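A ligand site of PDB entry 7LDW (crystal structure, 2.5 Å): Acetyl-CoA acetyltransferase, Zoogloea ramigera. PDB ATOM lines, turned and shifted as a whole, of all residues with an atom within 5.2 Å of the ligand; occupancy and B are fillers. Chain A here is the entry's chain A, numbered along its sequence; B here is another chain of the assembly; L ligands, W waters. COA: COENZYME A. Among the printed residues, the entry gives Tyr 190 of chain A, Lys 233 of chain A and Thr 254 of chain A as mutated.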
ATOM      1  N   SCY A  96       2.078 -18.863  -5.481  1.00  0.00           N
ATOM      2  CA  SCY A  96       2.188 -19.460  -6.811  1.00  0.00           C
ATOM      3  CB  SCY A  96       1.226 -18.798  -7.782  1.00  0.00           C
ATOM      4  SG  SCY A  96      -0.458 -18.967  -7.221  1.00  0.00           S
ATOM      5  CD  SCY A  96      -0.751 -17.696  -6.125  1.00  0.00           C
ATOM      6  OCD SCY A  96      -0.155 -16.619  -6.026  1.00  0.00           O
ATOM      7  CE  SCY A  96      -1.887 -18.045  -5.211  1.00  0.00           C
ATOM      8  C   SCY A  96       3.613 -19.420  -7.485  1.00  0.00           C
ATOM      9  O   SCY A  96       3.851 -20.172  -8.467  1.00  0.00           O
ATOM     10  N   LEU A 155      -6.092 -19.121  -1.558  1.00  0.00           N
ATOM     11  CA  LEU A 155      -6.885 -18.501  -2.605  1.00  0.00           C
ATOM     12  C   LEU A 155      -7.656 -17.267  -2.146  1.00  0.00           C
ATOM     13  O   LEU A 155      -8.530 -16.795  -2.885  1.00  0.00           O
ATOM     14  CB  LEU A 155      -7.856 -19.530  -3.200  1.00  0.00           C
ATOM     15  CG  LEU A 155      -7.226 -20.866  -3.595  1.00  0.00           C
ATOM     16  CD1 LEU A 155      -8.286 -21.849  -4.089  1.00  0.00           C
ATOM     17  CD2 LEU A 155      -6.135 -20.676  -4.639  1.00  0.00           C
ATOM     18  N   HIS A 163     -11.760 -13.738  -3.034  1.00  0.00           N
ATOM     19  CA  HIS A 163     -11.023 -14.782  -3.736  1.00  0.00           C
ATOM     20  C   HIS A 163     -10.083 -14.174  -4.782  1.00  0.00           C
ATOM     21  O   HIS A 163     -10.244 -13.015  -5.191  1.00  0.00           O
ATOM     22  CB  HIS A 163     -11.997 -15.759  -4.393  1.00  0.00           C
ATOM     23  CG  HIS A 163     -11.412 -17.090  -4.728  1.00  0.00           C
ATOM     24  ND1 HIS A 163     -10.626 -17.303  -5.839  1.00  0.00           N
ATOM     25  CD2 HIS A 163     -11.512 -18.290  -4.109  1.00  0.00           C
ATOM     26  CE1 HIS A 163     -10.264 -18.582  -5.881  1.00  0.00           C
ATOM     27  NE2 HIS A 163     -10.794 -19.198  -4.839  1.00  0.00           N
ATOM     28  N   MET A 164      -9.097 -14.967  -5.211  1.00  0.00           N
ATOM     29  CA  MET A 164      -8.207 -14.536  -6.286  1.00  0.00           C
ATOM     30  C   MET A 164      -8.970 -14.289  -7.584  1.00  0.00           C
ATOM     31  O   MET A 164      -8.532 -13.476  -8.406  1.00  0.00           O
ATOM     32  CB  MET A 164      -7.106 -15.566  -6.515  1.00  0.00           C
ATOM     33  CG  MET A 164      -6.128 -15.743  -5.351  1.00  0.00           C
ATOM     34  SD  MET A 164      -5.155 -14.262  -5.030  1.00  0.00           S
ATOM     35  CE  MET A 164      -6.069 -13.505  -3.688  1.00  0.00           C
ATOM     36  N   TYR A 190      -6.955 -24.988 -24.090  1.00  0.00           N
ATOM     37  CA  TYR A 190      -7.265 -26.417 -24.068  1.00  0.00           C
ATOM     38  C   TYR A 190      -6.811 -27.106 -25.338  1.00  0.00           C
ATOM     39  O   TYR A 190      -6.267 -28.218 -25.299  1.00  0.00           O
ATOM     40  CB  TYR A 190      -8.774 -26.612 -23.885  1.00  0.00           C
ATOM     41  CG  TYR A 190      -9.242 -26.577 -22.437  1.00  0.00           C
ATOM     42  CD1 TYR A 190      -9.178 -27.721 -21.642  1.00  0.00           C
ATOM     43  CD2 TYR A 190      -9.765 -25.418 -21.883  1.00  0.00           C
ATOM     44  CE1 TYR A 190      -9.613 -27.692 -20.328  1.00  0.00           C
ATOM     45  CE2 TYR A 190     -10.199 -25.389 -20.569  1.00  0.00           C
ATOM     46  CZ  TYR A 190     -10.114 -26.527 -19.799  1.00  0.00           C
ATOM     47  OH  TYR A 190     -10.552 -26.502 -18.498  1.00  0.00           O
ATOM     48  N   ALA A 229     -12.395 -28.992 -25.162  1.00  0.00           N
ATOM     49  CA  ALA A 229     -13.316 -27.927 -24.793  1.00  0.00           C
ATOM     50  C   ALA A 229     -13.943 -27.342 -26.041  1.00  0.00           C
ATOM     51  O   ALA A 229     -13.294 -27.215 -27.087  1.00  0.00           O
ATOM     52  CB  ALA A 229     -12.604 -26.829 -23.992  1.00  0.00           C
ATOM     53  N   LYS A 233     -20.136 -24.953 -24.947  1.00  0.00           N
ATOM     54  CA  LYS A 233     -20.229 -25.326 -23.537  1.00  0.00           C
ATOM     55  C   LYS A 233     -19.515 -24.316 -22.655  1.00  0.00           C
ATOM     56  O   LYS A 233     -19.887 -24.139 -21.486  1.00  0.00           O
ATOM     57  CB  LYS A 233     -19.643 -26.720 -23.316  1.00  0.00           C
ATOM     58  CG  LYS A 233     -20.475 -27.873 -23.865  1.00  0.00           C
ATOM     59  CD  LYS A 233     -19.817 -29.206 -23.562  1.00  0.00           C
ATOM     60  CE  LYS A 233     -20.352 -29.816 -22.271  1.00  0.00           C
ATOM     61  NZ  LYS A 233     -19.659 -31.098 -21.949  1.00  0.00           N
ATOM     62  N   MET A 234     -18.495 -23.638 -23.189  1.00  0.00           N
ATOM     63  CA  MET A 234     -17.763 -22.644 -22.408  1.00  0.00           C
ATOM     64  C   MET A 234     -18.616 -21.404 -22.172  1.00  0.00           C
ATOM     65  O   MET A 234     -18.578 -20.815 -21.085  1.00  0.00           O
ATOM     66  CB  MET A 234     -16.467 -22.283 -23.116  1.00  0.00           C
ATOM     67  CG  MET A 234     -15.529 -21.403 -22.315  1.00  0.00           C
ATOM     68  SD  MET A 234     -14.727 -22.320 -20.992  1.00  0.00           S
ATOM     69  CE  MET A 234     -13.961 -23.646 -21.919  1.00  0.00           C
ATOM     70  N   LEU A 237     -21.382 -21.350 -19.158  1.00  0.00           N
ATOM     71  CA  LEU A 237     -21.030 -21.431 -17.749  1.00  0.00           C
ATOM     72  C   LEU A 237     -21.348 -20.120 -17.031  1.00  0.00           C
ATOM     73  O   LEU A 237     -21.163 -19.037 -17.588  1.00  0.00           O
ATOM     74  CB  LEU A 237     -19.552 -21.771 -17.591  1.00  0.00           C
ATOM     75  CG  LEU A 237     -19.110 -23.112 -18.170  1.00  0.00           C
ATOM     76  CD1 LEU A 237     -17.607 -23.298 -18.005  1.00  0.00           C
ATOM     77  CD2 LEU A 237     -19.873 -24.242 -17.511  1.00  0.00           C
ATOM     78  N   ALA A 240     -18.216 -17.562 -11.565  1.00  0.00           N
ATOM     79  CA  ALA A 240     -17.938 -18.304 -10.345  1.00  0.00           C
ATOM     80  C   ALA A 240     -17.698 -17.421  -9.129  1.00  0.00           C
ATOM     81  O   ALA A 240     -17.730 -17.928  -8.002  1.00  0.00           O
ATOM     82  CB  ALA A 240     -16.719 -19.212 -10.544  1.00  0.00           C
ATOM     83  N   PHE A 241     -17.460 -16.121  -9.313  1.00  0.00           N
ATOM     84  CA  PHE A 241     -17.143 -15.226  -8.197  1.00  0.00           C
ATOM     85  C   PHE A 241     -18.129 -14.073  -8.123  1.00  0.00           C
ATOM     86  O   PHE A 241     -18.958 -14.045  -7.212  1.00  0.00           O
ATOM     87  CB  PHE A 241     -15.698 -14.738  -8.325  1.00  0.00           C
ATOM     88  CG  PHE A 241     -14.695 -15.853  -8.457  1.00  0.00           C
ATOM     89  CD1 PHE A 241     -14.299 -16.583  -7.351  1.00  0.00           C
ATOM     90  CD2 PHE A 241     -14.156 -16.184  -9.696  1.00  0.00           C
ATOM     91  CE1 PHE A 241     -13.372 -17.605  -7.469  1.00  0.00           C
ATOM     92  CE2 PHE A 241     -13.243 -17.205  -9.818  1.00  0.00           C
ATOM     93  CZ  PHE A 241     -12.848 -17.918  -8.701  1.00  0.00           C
ATOM     94  N   THR A 248     -15.289 -17.486 -15.033  1.00  0.00           N
ATOM     95  CA  THR A 248     -16.042 -18.711 -14.761  1.00  0.00           C
ATOM     96  C   THR A 248     -15.068 -19.830 -14.429  1.00  0.00           C
ATOM     97  O   THR A 248     -13.849 -19.666 -14.457  1.00  0.00           O
ATOM     98  CB  THR A 248     -16.919 -19.084 -15.967  1.00  0.00           C
ATOM     99  OG1 THR A 248     -16.091 -19.516 -17.046  1.00  0.00           O
ATOM    100  CG2 THR A 248     -17.754 -17.888 -16.416  1.00  0.00           C
ATOM    101  N   ALA A 249     -15.619 -21.000 -14.103  1.00  0.00           N
ATOM    102  CA  ALA A 249     -14.782 -22.164 -13.851  1.00  0.00           C
ATOM    103  C   ALA A 249     -14.072 -22.632 -15.113  1.00  0.00           C
ATOM    104  O   ALA A 249     -13.040 -23.323 -15.028  1.00  0.00           O
ATOM    105  CB  ALA A 249     -15.627 -23.305 -13.278  1.00  0.00           C
ATOM    106  N   GLY A 250     -14.580 -22.263 -16.286  1.00  0.00           N
ATOM    107  CA  GLY A 250     -13.979 -22.677 -17.536  1.00  0.00           C
ATOM    108  C   GLY A 250     -12.772 -21.860 -17.928  1.00  0.00           C
ATOM    109  O   GLY A 250     -11.767 -22.409 -18.416  1.00  0.00           O
ATOM    110  N   ALA A 252     -10.951 -20.081 -15.792  1.00  0.00           N
ATOM    111  CA  ALA A 252     -10.052 -19.978 -14.665  1.00  0.00           C
ATOM    112  C   ALA A 252      -9.334 -21.304 -14.454  1.00  0.00           C
ATOM    113  O   ALA A 252      -9.873 -22.369 -14.749  1.00  0.00           O
ATOM    114  CB  ALA A 252     -10.803 -19.588 -13.380  1.00  0.00           C
ATOM    115  N   SER A 253      -8.117 -21.227 -13.925  1.00  0.00           N
ATOM    116  CA  SER A 253      -7.373 -22.439 -13.612  1.00  0.00           C
ATOM    117  C   SER A 253      -8.077 -23.228 -12.511  1.00  0.00           C
ATOM    118  O   SER A 253      -8.890 -22.697 -11.748  1.00  0.00           O
ATOM    119  CB  SER A 253      -5.934 -22.094 -13.187  1.00  0.00           C
ATOM    120  OG  SER A 253      -5.923 -21.236 -12.057  1.00  0.00           O
ATOM    121  N   THR A 254      -7.735 -24.511 -12.421  1.00  0.00           N
ATOM    122  CA  THR A 254      -8.382 -25.411 -11.492  1.00  0.00           C
ATOM    123  C   THR A 254      -7.469 -25.685 -10.298  1.00  0.00           C
ATOM    124  O   THR A 254      -6.329 -25.217 -10.216  1.00  0.00           O
ATOM    125  CB  THR A 254      -8.760 -26.719 -12.201  1.00  0.00           C
ATOM    126  OG1 THR A 254      -7.669 -27.167 -12.999  1.00  0.00           O
ATOM    127  CG2 THR A 254      -9.980 -26.501 -13.094  1.00  0.00           C
ATOM    128  N   LEU A 255      -7.989 -26.459  -9.343  1.00  0.00           N
ATOM    129  CA  LEU A 255      -7.228 -26.885  -8.175  1.00  0.00           C
ATOM    130  C   LEU A 255      -6.645 -28.264  -8.455  1.00  0.00           C
ATOM    131  O   LEU A 255      -7.348 -29.164  -8.917  1.00  0.00           O
ATOM    132  CB  LEU A 255      -8.129 -26.918  -6.941  1.00  0.00           C
ATOM    133  CG  LEU A 255      -9.039 -25.708  -6.778  1.00  0.00           C
ATOM    134  CD1 LEU A 255      -9.955 -25.863  -5.577  1.00  0.00           C
ATOM    135  CD2 LEU A 255      -8.230 -24.431  -6.680  1.00  0.00           C
ATOM    136  N   MET A 294      -3.240  -8.374  -8.679  1.00  0.00           N
ATOM    137  CA  MET A 294      -2.057  -9.216  -8.545  1.00  0.00           C
ATOM    138  C   MET A 294      -1.700  -9.931  -9.844  1.00  0.00           C
ATOM    139  O   MET A 294      -0.546 -10.338 -10.014  1.00  0.00           O
ATOM    140  CB  MET A 294      -2.273 -10.240  -7.419  1.00  0.00           C
ATOM    141  CG  MET A 294      -3.348 -11.291  -7.700  1.00  0.00           C
ATOM    142  SD  MET A 294      -2.709 -12.791  -8.467  1.00  0.00           S
ATOM    143  CE  MET A 294      -4.226 -13.543  -9.050  1.00  0.00           C
ATOM    144  N   ALA A 324      -2.957 -18.148 -14.674  1.00  0.00           N
ATOM    145  CA  ALA A 324      -3.840 -18.287 -13.514  1.00  0.00           C
ATOM    146  C   ALA A 324      -5.289 -18.056 -13.905  1.00  0.00           C
ATOM    147  O   ALA A 324      -6.179 -18.804 -13.502  1.00  0.00           O
ATOM    148  CB  ALA A 324      -3.411 -17.311 -12.415  1.00  0.00           C
ATOM    149  N   PHE A 325      -5.549 -17.020 -14.709  1.00  0.00           N
ATOM    150  CA  PHE A 325      -6.863 -16.734 -15.241  1.00  0.00           C
ATOM    151  C   PHE A 325      -6.717 -16.263 -16.683  1.00  0.00           C
ATOM    152  O   PHE A 325      -5.680 -15.710 -17.059  1.00  0.00           O
ATOM    153  CB  PHE A 325      -7.604 -15.666 -14.428  1.00  0.00           C
ATOM    154  CG  PHE A 325      -7.836 -16.044 -12.994  1.00  0.00           C
ATOM    155  CD1 PHE A 325      -6.879 -15.789 -12.019  1.00  0.00           C
ATOM    156  CD2 PHE A 325      -9.018 -16.663 -12.610  1.00  0.00           C
ATOM    157  CE1 PHE A 325      -7.085 -16.143 -10.710  1.00  0.00           C
ATOM    158  CE2 PHE A 325      -9.227 -17.024 -11.290  1.00  0.00           C
ATOM    159  CZ  PHE A 325      -8.272 -16.765 -10.339  1.00  0.00           C
ATOM    160  N   HIS A 354      -3.047 -26.067 -12.097  1.00  0.00           N
ATOM    161  CA  HIS A 354      -2.310 -25.077 -11.309  1.00  0.00           C
ATOM    162  C   HIS A 354      -2.124 -25.587  -9.889  1.00  0.00           C
ATOM    163  O   HIS A 354      -2.848 -25.186  -8.968  1.00  0.00           O
ATOM    164  CB  HIS A 354      -3.031 -23.730 -11.331  1.00  0.00           C
ATOM    165  CG  HIS A 354      -2.199 -22.586 -10.841  1.00  0.00           C
ATOM    166  ND1 HIS A 354      -1.109 -22.742 -10.025  1.00  0.00           N
ATOM    167  CD2 HIS A 354      -2.307 -21.254 -11.065  1.00  0.00           C
ATOM    168  CE1 HIS A 354      -0.578 -21.566  -9.755  1.00  0.00           C
ATOM    169  NE2 HIS A 354      -1.286 -20.638 -10.381  1.00  0.00           N
ATOM    170  N   ILE A 356      -0.384 -24.908  -6.806  1.00  0.00           N
ATOM    171  CA  ILE A 356       0.182 -23.591  -6.491  1.00  0.00           C
ATOM    172  C   ILE A 356       1.667 -23.702  -6.149  1.00  0.00           C
ATOM    173  O   ILE A 356       2.506 -23.024  -6.746  1.00  0.00           O
ATOM    174  CB  ILE A 356      -0.624 -22.913  -5.363  1.00  0.00           C
ATOM    175  CG1 ILE A 356      -1.050 -23.926  -4.302  1.00  0.00           C
ATOM    176  CG2 ILE A 356      -1.835 -22.202  -5.946  1.00  0.00           C
ATOM    177  CD1 ILE A 356      -1.886 -23.320  -3.196  1.00  0.00           C
ATOM    178  N   CYS A 384       2.371 -14.831 -11.988  1.00  0.00           N
ATOM    179  CA  CYS A 384       1.797 -13.872 -11.057  1.00  0.00           C
ATOM    180  C   CYS A 384       1.620 -14.535  -9.692  1.00  0.00           C
ATOM    181  O   CYS A 384       1.415 -15.745  -9.587  1.00  0.00           O
ATOM    182  CB  CYS A 384       0.442 -13.357 -11.561  1.00  0.00           C
ATOM    183  SG  CYS A 384      -0.885 -14.566 -11.559  1.00  0.00           S
ATOM    184  N   GLY A 386      -0.137 -14.218  -5.708  1.00  0.00           N
ATOM    185  CA  GLY A 386      -1.132 -13.600  -4.863  1.00  0.00           C
ATOM    186  C   GLY A 386      -0.512 -12.618  -3.878  1.00  0.00           C
ATOM    187  O   GLY A 386       0.661 -12.712  -3.514  1.00  0.00           O
ATOM    188  N   LYS B 140     -16.081 -31.147   0.112  1.00  0.00           N
ATOM    189  CA  LYS B 140     -15.098 -31.051  -0.968  1.00  0.00           C
ATOM    190  C   LYS B 140     -14.373 -29.716  -0.953  1.00  0.00           C
ATOM    191  O   LYS B 140     -13.190 -29.658  -1.302  1.00  0.00           O
ATOM    192  CB  LYS B 140     -15.764 -31.280  -2.329  1.00  0.00           C
ATOM    193  CG  LYS B 140     -16.652 -30.146  -2.819  1.00  0.00           C
ATOM    194  CD  LYS B 140     -16.811 -30.181  -4.335  1.00  0.00           C
ATOM    195  CE  LYS B 140     -15.508 -29.833  -5.041  1.00  0.00           C
ATOM    196  NZ  LYS B 140     -15.647 -29.877  -6.521  1.00  0.00           N
ATOM    197  N   MET B 141     -15.047 -28.642  -0.547  1.00  0.00           N
ATOM    198  CA  MET B 141     -14.457 -27.309  -0.549  1.00  0.00           C
ATOM    199  C   MET B 141     -15.323 -26.383   0.280  1.00  0.00           C
ATOM    200  O   MET B 141     -16.542 -26.574   0.387  1.00  0.00           O
ATOM    201  CB  MET B 141     -14.331 -26.783  -1.986  1.00  0.00           C
ATOM    202  CG  MET B 141     -13.512 -25.516  -2.130  1.00  0.00           C
ATOM    203  SD  MET B 141     -13.373 -25.039  -3.860  1.00  0.00           S
ATOM    204  CE  MET B 141     -15.087 -24.821  -4.305  1.00  0.00           C
HETATM  205  N1A COA L   1     -15.500 -26.566 -20.119  1.00  0.00           N
HETATM  206  C2A COA L   1     -16.817 -26.635 -19.994  1.00  0.00           C
HETATM  207  N3A COA L   1     -17.440 -26.717 -18.831  1.00  0.00           N
HETATM  208  C4A COA L   1     -16.719 -26.718 -17.696  1.00  0.00           C
HETATM  209  C5A COA L   1     -15.334 -26.654 -17.804  1.00  0.00           C
HETATM  210  C6A COA L   1     -14.729 -26.577 -19.037  1.00  0.00           C
HETATM  211  N6A COA L   1     -13.364 -26.514 -19.037  1.00  0.00           N
HETATM  212  N7A COA L   1     -14.793 -26.676 -16.571  1.00  0.00           N
HETATM  213  C8A COA L   1     -15.747 -26.754 -15.717  1.00  0.00           C
HETATM  214  N9A COA L   1     -16.958 -26.781 -16.342  1.00  0.00           N
HETATM  215  C1B COA L   1     -18.247 -26.873 -15.643  1.00  0.00           C
HETATM  216  C2B COA L   1     -18.282 -28.129 -14.725  1.00  0.00           C
HETATM  217  O2B COA L   1     -18.735 -29.347 -15.343  1.00  0.00           O
HETATM  218  C3B COA L   1     -19.261 -27.659 -13.613  1.00  0.00           C
HETATM  219  O3B COA L   1     -20.620 -27.650 -14.074  1.00  0.00           O
HETATM  220  P3B COA L   1     -21.477 -28.774 -13.308  1.00  0.00           P
HETATM  221  O7A COA L   1     -22.889 -28.342 -13.323  1.00  0.00           O
HETATM  222  O8A COA L   1     -21.327 -30.195 -14.083  1.00  0.00           O
HETATM  223  O9A COA L   1     -20.980 -28.917 -11.766  1.00  0.00           O
HETATM  224  C4B COA L   1     -18.777 -26.211 -13.420  1.00  0.00           C
HETATM  225  O4B COA L   1     -18.412 -25.751 -14.723  1.00  0.00           O
HETATM  226  C5B COA L   1     -17.525 -26.186 -12.529  1.00  0.00           C
HETATM  227  O5B COA L   1     -17.609 -27.098 -11.428  1.00  0.00           O
HETATM  228  P1A COA L   1     -16.093 -27.502 -11.037  1.00  0.00           P
HETATM  229  O1A COA L   1     -15.436 -28.051 -12.256  1.00  0.00           O
HETATM  230  O2A COA L   1     -16.136 -28.676  -9.916  1.00  0.00           O
HETATM  231  O3A COA L   1     -15.187 -26.254 -10.551  1.00  0.00           O
HETATM  232  P2A COA L   1     -15.705 -25.577  -9.178  1.00  0.00           P
HETATM  233  O4A COA L   1     -17.035 -24.989  -9.440  1.00  0.00           O
HETATM  234  O5A COA L   1     -15.820 -26.699  -8.017  1.00  0.00           O
HETATM  235  O6A COA L   1     -14.685 -24.424  -8.677  1.00  0.00           O
HETATM  236  CBP COA L   1     -13.140 -22.667  -9.290  1.00  0.00           C
HETATM  237  CCP COA L   1     -14.040 -23.806  -9.797  1.00  0.00           C
HETATM  238  CDP COA L   1     -12.872 -21.676 -10.430  1.00  0.00           C
HETATM  239  CEP COA L   1     -13.895 -21.937  -8.180  1.00  0.00           C
HETATM  240  CAP COA L   1     -11.808 -23.221  -8.766  1.00  0.00           C
HETATM  241  OAP COA L   1     -11.176 -23.973  -9.804  1.00  0.00           O
HETATM  242  C9P COA L   1     -10.832 -22.167  -8.266  1.00  0.00           C
HETATM  243  O9P COA L   1     -10.983 -21.665  -7.180  1.00  0.00           O
HETATM  244  N8P COA L   1      -9.768 -21.783  -9.003  1.00  0.00           N
HETATM  245  C7P COA L   1      -8.855 -20.768  -8.470  1.00  0.00           C
HETATM  246  C6P COA L   1      -7.498 -20.813  -9.188  1.00  0.00           C
HETATM  247  C5P COA L   1      -6.499 -19.908  -8.509  1.00  0.00           C
HETATM  248  O5P COA L   1      -6.863 -19.132  -7.655  1.00  0.00           O
HETATM  249  N4P COA L   1      -5.192 -19.958  -8.858  1.00  0.00           N
HETATM  250  C3P COA L   1      -4.193 -19.099  -8.219  1.00  0.00           C
HETATM  251  C2P COA L   1      -4.326 -17.657  -8.711  1.00  0.00           C
HETATM  252  S1P COA L   1      -2.683 -16.881  -8.848  1.00  0.00           S
HETATM  253  O   HOH W   1     -11.614 -23.648 -12.965  1.00  0.00           O
HETATM  254  O   HOH W   2     -13.631 -28.224  -8.126  1.00  0.00           O
HETATM  255  O   HOH W   3     -12.352 -26.080 -15.381  1.00  0.00           O
HETATM  256  O   HOH W   4     -16.332 -30.366 -17.123  1.00  0.00           O
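SG of SCY 96 sits close to S1P of the ligand, 3.5 Å away.
O9P of the ligand lies within hydrogen-bond range of NE2 of His 163 (3.4 Å).
The side-chain hydroxyl of Tyr 190 sits at hydrogen-bond distance from a nitrogen (N6A) of the ligand, at 2.9 Å.
An oxygen (O5A) of the ligand is in salt-bridge range of the side-chain amino group of Lys 140 of chain B (3.5 Å).
The backbone carbonyl oxygen (O) of Ser 253 sits at hydrogen-bond distance from a nitrogen (N8P) of the ligand, 3.0 Å away.
The backbone NH (N) of Gly 386 sits at hydrogen-bond distance from OCD of SCY 96 (2.4 Å).
SG of SCY 96 sits close to a ring nitrogen (NE2) of His 354 (3.7 Å).
The side-chain hydroxyl of Ser 253 sits at hydrogen-bond distance from the backbone carbonyl oxygen of Ala 324 (2.8 Å).
O of Leu 155 sits at hydrogen-bond distance from N of Met 164, at 3.0 Å.
Residues that only touch the ligand: Leu 155 (3.5 Å), Leu 237 (3.5 Å), Ala 249 (3.5 Å), Thr 254 (3.6 Å), Ala 324 (3.7 Å), Met 294 (3.7 Å), Phe 325 (3.7 Å), Met 164 (3.8 Å), Met 234 (3.8 Å), Leu 255 (3.8 Å), His 354 (3.9 Å) and Cys 384 (3.99 Å).
Hydrophobic or aromatic side chains within 4 Å of the ligand: Leu 155, His 163, Met 164, Tyr 190, Met 234, Leu 237, Ala 249, Leu 255, Met 294, Ala 324, Phe 325 and His 354.
Along chain A the residues within 4 Å of the ligand span positions 96 to 384.
Water W2 bridges O5A of the ligand (2.7 Å) and NZ of Lys 140 of chain B (3.1 Å).
Water W3 bridges a nitrogen (N7A) of the ligand and the backbone carbonyl oxygen (O) of Ala 249.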
